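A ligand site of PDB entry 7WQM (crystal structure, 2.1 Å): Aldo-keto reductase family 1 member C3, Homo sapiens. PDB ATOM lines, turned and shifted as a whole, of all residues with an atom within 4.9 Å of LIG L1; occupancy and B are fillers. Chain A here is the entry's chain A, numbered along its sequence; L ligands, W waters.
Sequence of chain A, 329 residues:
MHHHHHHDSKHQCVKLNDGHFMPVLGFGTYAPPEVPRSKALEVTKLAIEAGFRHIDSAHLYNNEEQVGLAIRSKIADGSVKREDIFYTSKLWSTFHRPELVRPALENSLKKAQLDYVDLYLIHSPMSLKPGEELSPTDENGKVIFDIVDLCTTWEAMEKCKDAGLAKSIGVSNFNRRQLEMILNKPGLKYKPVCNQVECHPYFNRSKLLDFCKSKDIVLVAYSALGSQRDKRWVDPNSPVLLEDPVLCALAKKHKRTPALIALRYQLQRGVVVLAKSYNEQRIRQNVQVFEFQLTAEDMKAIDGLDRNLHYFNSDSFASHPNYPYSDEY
An oxygen (O3) of LIG L1 lies within hydrogen-bond range of the side-chain hydroxyl (OG) of Ser 124 (3.0 Å). The side-chain amide nitrogen of Asn 173 lies close to an oxygen (O3) of LIG L1 (3.4 Å). The side-chain amide nitrogen (ND2) of Asn 173 lies within hydrogen-bond range of an oxygen (O14) of LG2 L2, 2.9 Å away. NE2 of His 123 lies within hydrogen-bond range of O14 of LG2 L2. An oxygen (O10) of LG2 L2 lies within hydrogen-bond range of the backbone NH of Ser 223 (3.1 Å). The side-chain hydroxyl (OG) of Ser 223 lies within hydrogen-bond range of an oxygen (O9) of LG2 L2 (2.7 Å).
OG of Ser 124 lies within hydrogen-bond range of N of Met 126, at 3.1 Å. OD1 of Asn 173 sits at hydrogen-bond distance from OH of Tyr 222, 2.5 Å away. ND2 of Asn 173 lies within hydrogen-bond range of O of His 123 (2.9 Å).
Merely in contact with LIG L1: Leu 60 (3.96 Å), Trp 92 (3.5 Å), Met 126 (3.3 Å), Ser 135 (3.6 Å), Tyr 222 (3.6 Å), Trp 233 (3.7 Å), Phe 312 (3.4 Å), Phe 317 (3.5 Å) and Tyr 325 (3.9 Å). Hydrophobic or aromatic side chains within 4 Å of LIG L1: Leu 60, Trp 92, Met 126, Trp 233, Phe 312, Phe 317 and Tyr 325. Within 4 Å of LIG L1: Leu 60, Trp 92, Ser 124, Met 126, Ser 135, Asn 173, Tyr 222, Trp 233, Phe 312, Phe 317 and Tyr 325. The nearest printed residue that does not touch LIG L1 is His 123 (4.04 Å).
Water W1 lies within hydrogen-bond range of the side-chain hydroxyl (OH) of Tyr 325 and the side-chain hydroxyl (OH) of Tyr 222.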
ATOM      1  N   LEU A  60       1.891  -2.422   7.069  1.00  0.00           N
ATOM      2  CA  LEU A  60       0.993  -3.235   6.249  1.00  0.00           C
ATOM      3  C   LEU A  60      -0.012  -2.383   5.479  1.00  0.00           C
ATOM      4  O   LEU A  60      -0.430  -2.769   4.380  1.00  0.00           O
ATOM      5  CB  LEU A  60       0.256  -4.241   7.142  1.00  0.00           C
ATOM      6  CG  LEU A  60      -0.846  -5.081   6.515  1.00  0.00           C
ATOM      7  CD1 LEU A  60      -0.267  -6.066   5.518  1.00  0.00           C
ATOM      8  CD2 LEU A  60      -1.674  -5.803   7.580  1.00  0.00           C
ATOM      9  N   TRP A  92       5.704  -5.078  10.658  1.00  0.00           N
ATOM     10  CA  TRP A  92       5.037  -6.164   9.960  1.00  0.00           C
ATOM     11  C   TRP A  92       5.746  -7.491  10.194  1.00  0.00           C
ATOM     12  O   TRP A  92       6.920  -7.541  10.572  1.00  0.00           O
ATOM     13  CB  TRP A  92       4.919  -5.873   8.458  1.00  0.00           C
ATOM     14  CG  TRP A  92       4.112  -6.935   7.738  1.00  0.00           C
ATOM     15  CD1 TRP A  92       4.485  -7.626   6.618  1.00  0.00           C
ATOM     16  CD2 TRP A  92       2.830  -7.451   8.121  1.00  0.00           C
ATOM     17  NE1 TRP A  92       3.503  -8.524   6.276  1.00  0.00           N
ATOM     18  CE2 TRP A  92       2.473  -8.430   7.180  1.00  0.00           C
ATOM     19  CE3 TRP A  92       1.935  -7.167   9.165  1.00  0.00           C
ATOM     20  CZ2 TRP A  92       1.276  -9.133   7.242  1.00  0.00           C
ATOM     21  CZ3 TRP A  92       0.746  -7.863   9.230  1.00  0.00           C
ATOM     22  CH2 TRP A  92       0.429  -8.835   8.280  1.00  0.00           C
ATOM     23  N   HIS A 123       2.847  -6.262  14.969  1.00  0.00           N
ATOM     24  CA  HIS A 123       1.524  -6.310  14.361  1.00  0.00           C
ATOM     25  C   HIS A 123       0.819  -7.640  14.605  1.00  0.00           C
ATOM     26  O   HIS A 123      -0.404  -7.672  14.746  1.00  0.00           O
ATOM     27  CB  HIS A 123       1.630  -6.048  12.860  1.00  0.00           C
ATOM     28  CG  HIS A 123       0.376  -5.517  12.242  1.00  0.00           C
ATOM     29  ND1 HIS A 123       0.375  -4.643  11.177  1.00  0.00           N
ATOM     30  CD2 HIS A 123      -0.927  -5.746  12.543  1.00  0.00           C
ATOM     31  CE1 HIS A 123      -0.877  -4.355  10.847  1.00  0.00           C
ATOM     32  NE2 HIS A 123      -1.682  -5.011  11.668  1.00  0.00           N
ATOM     33  N   SER A 124       1.566  -8.726  14.687  1.00  0.00           N
ATOM     34  CA  SER A 124       0.989 -10.054  14.798  1.00  0.00           C
ATOM     35  C   SER A 124       2.038 -11.036  15.288  1.00  0.00           C
ATOM     36  O   SER A 124       3.226 -10.853  14.990  1.00  0.00           O
ATOM     37  CB  SER A 124       0.422 -10.498  13.456  1.00  0.00           C
ATOM     38  OG  SER A 124       0.309 -11.904  13.379  1.00  0.00           O
ATOM     39  N   MET A 126       2.366 -14.078  14.275  1.00  0.00           N
ATOM     40  CA  MET A 126       2.561 -15.095  13.252  1.00  0.00           C
ATOM     41  C   MET A 126       3.634 -14.621  12.286  1.00  0.00           C
ATOM     42  O   MET A 126       3.370 -13.855  11.360  1.00  0.00           O
ATOM     43  CB  MET A 126       1.242 -15.396  12.541  1.00  0.00           C
ATOM     44  CG  MET A 126       0.177 -15.971  13.467  1.00  0.00           C
ATOM     45  SD  MET A 126      -1.349 -16.443  12.644  1.00  0.00           S
ATOM     46  CE  MET A 126      -2.158 -14.855  12.490  1.00  0.00           C
ATOM     47  N   LEU A 128       6.411 -14.359   9.348  1.00  0.00           N
ATOM     48  CA  LEU A 128       6.415 -14.730   7.943  1.00  0.00           C
ATOM     49  C   LEU A 128       7.827 -14.572   7.383  1.00  0.00           C
ATOM     50  O   LEU A 128       8.697 -13.950   7.987  1.00  0.00           O
ATOM     51  CB  LEU A 128       5.438 -13.882   7.117  1.00  0.00           C
ATOM     52  CG  LEU A 128       3.980 -13.843   7.578  1.00  0.00           C
ATOM     53  CD1 LEU A 128       3.207 -12.829   6.756  1.00  0.00           C
ATOM     54  CD2 LEU A 128       3.337 -15.224   7.469  1.00  0.00           C
ATOM     55  N   SER A 135       3.116 -10.643   1.893  1.00  0.00           N
ATOM     56  CA  SER A 135       2.571 -11.997   2.017  1.00  0.00           C
ATOM     57  C   SER A 135       3.389 -12.929   1.137  1.00  0.00           C
ATOM     58  O   SER A 135       2.967 -13.291   0.031  1.00  0.00           O
ATOM     59  CB  SER A 135       1.097 -12.037   1.635  1.00  0.00           C
ATOM     60  OG  SER A 135       0.283 -11.523   2.673  1.00  0.00           O
ATOM     61  N   ASN A 173      -2.683  -8.591  18.474  1.00  0.00           N
ATOM     62  CA  ASN A 173      -3.174  -9.937  18.150  1.00  0.00           C
ATOM     63  C   ASN A 173      -2.503 -11.027  18.971  1.00  0.00           C
ATOM     64  O   ASN A 173      -2.427 -12.184  18.552  1.00  0.00           O
ATOM     65  CB  ASN A 173      -3.017 -10.242  16.651  1.00  0.00           C
ATOM     66  CG  ASN A 173      -3.850  -9.322  15.773  1.00  0.00           C
ATOM     67  OD1 ASN A 173      -5.073  -9.261  15.890  1.00  0.00           O
ATOM     68  ND2 ASN A 173      -3.177  -8.598  14.888  1.00  0.00           N
ATOM     69  N   TYR A 222      -9.744  -3.109  17.815  1.00  0.00           N
ATOM     70  CA  TYR A 222      -9.981  -2.840  16.403  1.00  0.00           C
ATOM     71  C   TYR A 222     -11.180  -3.654  15.935  1.00  0.00           C
ATOM     72  O   TYR A 222     -11.629  -4.574  16.617  1.00  0.00           O
ATOM     73  CB  TYR A 222      -8.733  -3.141  15.546  1.00  0.00           C
ATOM     74  CG  TYR A 222      -8.357  -4.599  15.368  1.00  0.00           C
ATOM     75  CD1 TYR A 222      -9.110  -5.457  14.567  1.00  0.00           C
ATOM     76  CD2 TYR A 222      -7.214  -5.109  15.971  1.00  0.00           C
ATOM     77  CE1 TYR A 222      -8.745  -6.778  14.393  1.00  0.00           C
ATOM     78  CE2 TYR A 222      -6.841  -6.424  15.800  1.00  0.00           C
ATOM     79  CZ  TYR A 222      -7.617  -7.261  15.007  1.00  0.00           C
ATOM     80  OH  TYR A 222      -7.258  -8.575  14.833  1.00  0.00           O
ATOM     81  N   SER A 223     -11.703  -3.282  14.763  1.00  0.00           N
ATOM     82  CA  SER A 223     -12.954  -3.823  14.252  1.00  0.00           C
ATOM     83  C   SER A 223     -14.095  -3.637  15.252  1.00  0.00           C
ATOM     84  O   SER A 223     -15.037  -4.423  15.291  1.00  0.00           O
ATOM     85  CB  SER A 223     -12.814  -5.309  13.868  1.00  0.00           C
ATOM     86  OG  SER A 223     -11.944  -5.469  12.759  1.00  0.00           O
ATOM     87  N   TRP A 233     -11.776 -11.581   3.164  1.00  0.00           N
ATOM     88  CA  TRP A 233     -11.747 -12.411   4.394  1.00  0.00           C
ATOM     89  C   TRP A 233     -13.146 -12.637   4.965  1.00  0.00           C
ATOM     90  O   TRP A 233     -13.582 -13.790   5.043  1.00  0.00           O
ATOM     91  CB  TRP A 233     -10.894 -11.763   5.485  1.00  0.00           C
ATOM     92  CG  TRP A 233      -9.760 -10.887   5.030  1.00  0.00           C
ATOM     93  CD1 TRP A 233      -9.807  -9.566   4.719  1.00  0.00           C
ATOM     94  CD2 TRP A 233      -8.390 -11.286   4.882  1.00  0.00           C
ATOM     95  NE1 TRP A 233      -8.570  -9.118   4.352  1.00  0.00           N
ATOM     96  CE2 TRP A 233      -7.682 -10.159   4.439  1.00  0.00           C
ATOM     97  CE3 TRP A 233      -7.702 -12.501   5.038  1.00  0.00           C
ATOM     98  CZ2 TRP A 233      -6.313 -10.202   4.185  1.00  0.00           C
ATOM     99  CZ3 TRP A 233      -6.347 -12.544   4.781  1.00  0.00           C
ATOM    100  CH2 TRP A 233      -5.666 -11.399   4.365  1.00  0.00           C
ATOM    101  N   PHE A 312     -11.985 -11.588  11.404  1.00  0.00           N
ATOM    102  CA  PHE A 312     -10.807 -12.145  10.708  1.00  0.00           C
ATOM    103  C   PHE A 312     -11.000 -13.650  10.568  1.00  0.00           C
ATOM    104  O   PHE A 312     -11.178 -14.335  11.561  1.00  0.00           O
ATOM    105  CB  PHE A 312      -9.505 -11.845  11.456  1.00  0.00           C
ATOM    106  CG  PHE A 312      -8.310 -12.569  10.899  1.00  0.00           C
ATOM    107  CD1 PHE A 312      -7.577 -12.023   9.857  1.00  0.00           C
ATOM    108  CD2 PHE A 312      -7.953 -13.813  11.372  1.00  0.00           C
ATOM    109  CE1 PHE A 312      -6.471 -12.691   9.351  1.00  0.00           C
ATOM    110  CE2 PHE A 312      -6.847 -14.480  10.866  1.00  0.00           C
ATOM    111  CZ  PHE A 312      -6.107 -13.913   9.862  1.00  0.00           C
ATOM    112  N   PHE A 317      -3.783 -19.210   7.938  1.00  0.00           N
ATOM    113  CA  PHE A 317      -2.994 -18.868   9.148  1.00  0.00           C
ATOM    114  C   PHE A 317      -3.448 -19.725  10.307  1.00  0.00           C
ATOM    115  O   PHE A 317      -2.754 -19.792  11.313  1.00  0.00           O
ATOM    116  CB  PHE A 317      -3.092 -17.374   9.483  1.00  0.00           C
ATOM    117  CG  PHE A 317      -2.432 -16.519   8.432  1.00  0.00           C
ATOM    118  CD1 PHE A 317      -1.070 -16.512   8.281  1.00  0.00           C
ATOM    119  CD2 PHE A 317      -3.206 -15.801   7.538  1.00  0.00           C
ATOM    120  CE1 PHE A 317      -0.477 -15.768   7.285  1.00  0.00           C
ATOM    121  CE2 PHE A 317      -2.606 -15.050   6.545  1.00  0.00           C
ATOM    122  CZ  PHE A 317      -1.237 -15.037   6.429  1.00  0.00           C
ATOM    123  N   PRO A 324      -3.312 -17.088  17.136  1.00  0.00           N
ATOM    124  CA  PRO A 324      -3.673 -16.699  18.513  1.00  0.00           C
ATOM    125  C   PRO A 324      -5.014 -17.211  18.987  1.00  0.00           C
ATOM    126  O   PRO A 324      -5.230 -17.284  20.202  1.00  0.00           O
ATOM    127  CB  PRO A 324      -3.679 -15.163  18.437  1.00  0.00           C
ATOM    128  CG  PRO A 324      -4.044 -14.859  17.019  1.00  0.00           C
ATOM    129  CD  PRO A 324      -3.545 -16.003  16.167  1.00  0.00           C
ATOM    130  N   TYR A 325      -5.883 -17.549  18.041  1.00  0.00           N
ATOM    131  CA  TYR A 325      -7.236 -18.089  18.316  1.00  0.00           C
ATOM    132  C   TYR A 325      -7.129 -19.620  18.283  1.00  0.00           C
ATOM    133  O   TYR A 325      -7.818 -20.269  19.052  1.00  0.00           O
ATOM    134  CB  TYR A 325      -8.254 -17.576  17.304  1.00  0.00           C
ATOM    135  CG  TYR A 325      -8.345 -16.077  17.145  1.00  0.00           C
ATOM    136  CD1 TYR A 325      -8.274 -15.210  18.219  1.00  0.00           C
ATOM    137  CD2 TYR A 325      -8.538 -15.524  15.888  1.00  0.00           C
ATOM    138  CE1 TYR A 325      -8.347 -13.841  18.059  1.00  0.00           C
ATOM    139  CE2 TYR A 325      -8.616 -14.160  15.715  1.00  0.00           C
ATOM    140  CZ  TYR A 325      -8.517 -13.310  16.793  1.00  0.00           C
ATOM    141  OH  TYR A 325      -8.624 -11.984  16.604  1.00  0.00           O
HETATM  142  N1  LIG L   1      -4.389  -9.399   7.980  1.00  0.00           N
HETATM  143  C1  LIG L   1      -8.758  -7.601   9.913  1.00  0.00           C
HETATM  144  C2  LIG L   1      -8.608  -7.148   8.621  1.00  0.00           C
HETATM  145  C3  LIG L   1      -7.444  -7.424   7.937  1.00  0.00           C
HETATM  146  C4  LIG L   1      -5.216  -8.379   7.641  1.00  0.00           C
HETATM  147  C5  LIG L   1      -3.329  -9.955   7.231  1.00  0.00           C
HETATM  148  C6  LIG L   1      -1.625 -11.670   7.124  1.00  0.00           C
HETATM  149  C7  LIG L   1      -2.913  -9.493   5.992  1.00  0.00           C
HETATM  150  C8  LIG L   1      -4.567 -10.466  12.294  1.00  0.00           C
HETATM  151  C9  LIG L   1      -4.581 -11.571  13.160  1.00  0.00           C
HETATM  152  C10 LIG L   1      -2.548 -12.579   9.645  1.00  0.00           C
HETATM  153  C11 LIG L   1      -6.410  -8.150   8.519  1.00  0.00           C
HETATM  154  C12 LIG L   1      -1.224 -11.195   5.894  1.00  0.00           C
HETATM  155  C13 LIG L   1      -1.859 -10.105   5.336  1.00  0.00           C
HETATM  156  C14 LIG L   1      -5.770  -9.755  11.770  1.00  0.00           C
HETATM  157  C15 LIG L   1      -3.264 -10.209  12.031  1.00  0.00           C
HETATM  158  C16 LIG L   1      -5.740 -12.278  13.770  1.00  0.00           C
HETATM  159  C17 LIG L   1      -2.533  -9.206  11.220  1.00  0.00           C
HETATM  160  C18 LIG L   1      -6.596  -8.621   9.829  1.00  0.00           C
HETATM  161  C19 LIG L   1      -7.766  -8.337  10.513  1.00  0.00           C
HETATM  162  C20 LIG L   1      -2.677 -11.070   7.799  1.00  0.00           C
HETATM  163  N2  LIG L   1      -3.365 -11.961  13.427  1.00  0.00           N
HETATM  164  O1  LIG L   1      -5.573  -9.343  10.397  1.00  0.00           O
HETATM  165  O2  LIG L   1      -5.040  -7.667   6.663  1.00  0.00           O
HETATM  166  O3  LIG L   1      -2.502 -11.104  12.706  1.00  0.00           O
HETATM  167  O4  LIG L   1      -3.155 -11.453   9.018  1.00  0.00           O
HETATM  168  P1  LG2 L   2     -14.011  -0.494  11.931  1.00  0.00           P
HETATM  169  O1  LG2 L   2     -14.522  -1.747  12.624  1.00  0.00           O
HETATM  170  O2  LG2 L   2     -13.525   0.523  12.978  1.00  0.00           O
HETATM  171  O3  LG2 L   2     -15.277   0.167  11.084  1.00  0.00           O
HETATM  172  C1  LG2 L   2     -15.912  -0.725  10.149  1.00  0.00           C
HETATM  173  C2  LG2 L   2     -16.829   0.094   9.217  1.00  0.00           C
HETATM  174  O4  LG2 L   2     -17.683   0.790   9.955  1.00  0.00           O
HETATM  175  C3  LG2 L   2     -15.974   1.156   8.515  1.00  0.00           C
HETATM  176  O5  LG2 L   2     -15.617   0.742   7.290  1.00  0.00           O
HETATM  177  C4  LG2 L   2     -16.922   2.410   8.392  1.00  0.00           C
HETATM  178  O6  LG2 L   2     -17.330   2.595   6.959  1.00  0.00           O
HETATM  179  C5  LG2 L   2     -17.983   2.152   9.120  1.00  0.00           C
HETATM  180  N1  LG2 L   2     -18.182   3.255  10.012  1.00  0.00           N
HETATM  181  C6  LG2 L   2     -17.323   4.081  10.645  1.00  0.00           C
HETATM  182  N2  LG2 L   2     -18.041   4.962  11.372  1.00  0.00           N
HETATM  183  C7  LG2 L   2     -19.351   4.686  11.186  1.00  0.00           C
HETATM  184  C8  LG2 L   2     -20.485   5.276  11.689  1.00  0.00           C
HETATM  185  N3  LG2 L   2     -20.570   6.412  12.608  1.00  0.00           N
HETATM  186  N4  LG2 L   2     -21.694   4.804  11.353  1.00  0.00           N
HETATM  187  C9  LG2 L   2     -21.795   3.745  10.506  1.00  0.00           C
HETATM  188  N5  LG2 L   2     -20.683   3.162  10.008  1.00  0.00           N
HETATM  189  C10 LG2 L   2     -19.454   3.639  10.352  1.00  0.00           C
HETATM  190  O7  LG2 L   2     -12.786  -0.848  10.825  1.00  0.00           O
HETATM  191  P2  LG2 L   2     -11.536  -1.875  11.023  1.00  0.00           P
HETATM  192  O8  LG2 L   2     -10.606  -1.744   9.863  1.00  0.00           O
HETATM  193  O9  LG2 L   2     -12.000  -3.292  11.092  1.00  0.00           O
HETATM  194  O10 LG2 L   2     -10.727  -1.457  12.413  1.00  0.00           O
HETATM  195  C11 LG2 L   2     -10.454  -0.039  12.641  1.00  0.00           C
HETATM  196  C12 LG2 L   2      -8.918   0.206  12.670  1.00  0.00           C
HETATM  197  O11 LG2 L   2      -8.351  -0.684  13.452  1.00  0.00           O
HETATM  198  C13 LG2 L   2      -8.296  -0.074  11.281  1.00  0.00           C
HETATM  199  O12 LG2 L   2      -8.368   1.010  10.461  1.00  0.00           O
HETATM  200  C14 LG2 L   2      -6.839  -0.422  11.653  1.00  0.00           C
HETATM  201  O13 LG2 L   2      -6.100   0.873  11.906  1.00  0.00           O
HETATM  202  C15 LG2 L   2      -6.936  -1.099  12.765  1.00  0.00           C
HETATM  203  N6  LG2 L   2      -6.861  -2.544  12.571  1.00  0.00           N
HETATM  204  C16 LG2 L   2      -5.825  -3.228  13.130  1.00  0.00           C
HETATM  205  C17 LG2 L   2      -5.710  -4.609  12.972  1.00  0.00           C
HETATM  206  C18 LG2 L   2      -4.536  -5.356  13.598  1.00  0.00           C
HETATM  207  O14 LG2 L   2      -4.287  -6.467  13.235  1.00  0.00           O
HETATM  208  N7  LG2 L   2      -3.738  -4.732  14.637  1.00  0.00           N
HETATM  209  C19 LG2 L   2      -6.649  -5.281  12.244  1.00  0.00           C
HETATM  210  C20 LG2 L   2      -7.685  -4.611  11.682  1.00  0.00           C
HETATM  211  C21 LG2 L   2      -7.782  -3.226  11.857  1.00  0.00           C
HETATM  212  P3  LG2 L   2     -17.022   4.069   6.247  1.00  0.00           P
HETATM  213  O15 LG2 L   2     -15.569   4.179   5.973  1.00  0.00           O
HETATM  214  O16 LG2 L   2     -17.785   4.173   4.945  1.00  0.00           O
HETATM  215  O17 LG2 L   2     -17.455   5.180   7.173  1.00  0.00           O
HETATM  216  O   HOH W   1      -8.831 -11.114  14.374  1.00  0.00           O
HETATM  217  O   HOH W   2     -11.582  -8.095  11.788  1.00  0.00           O
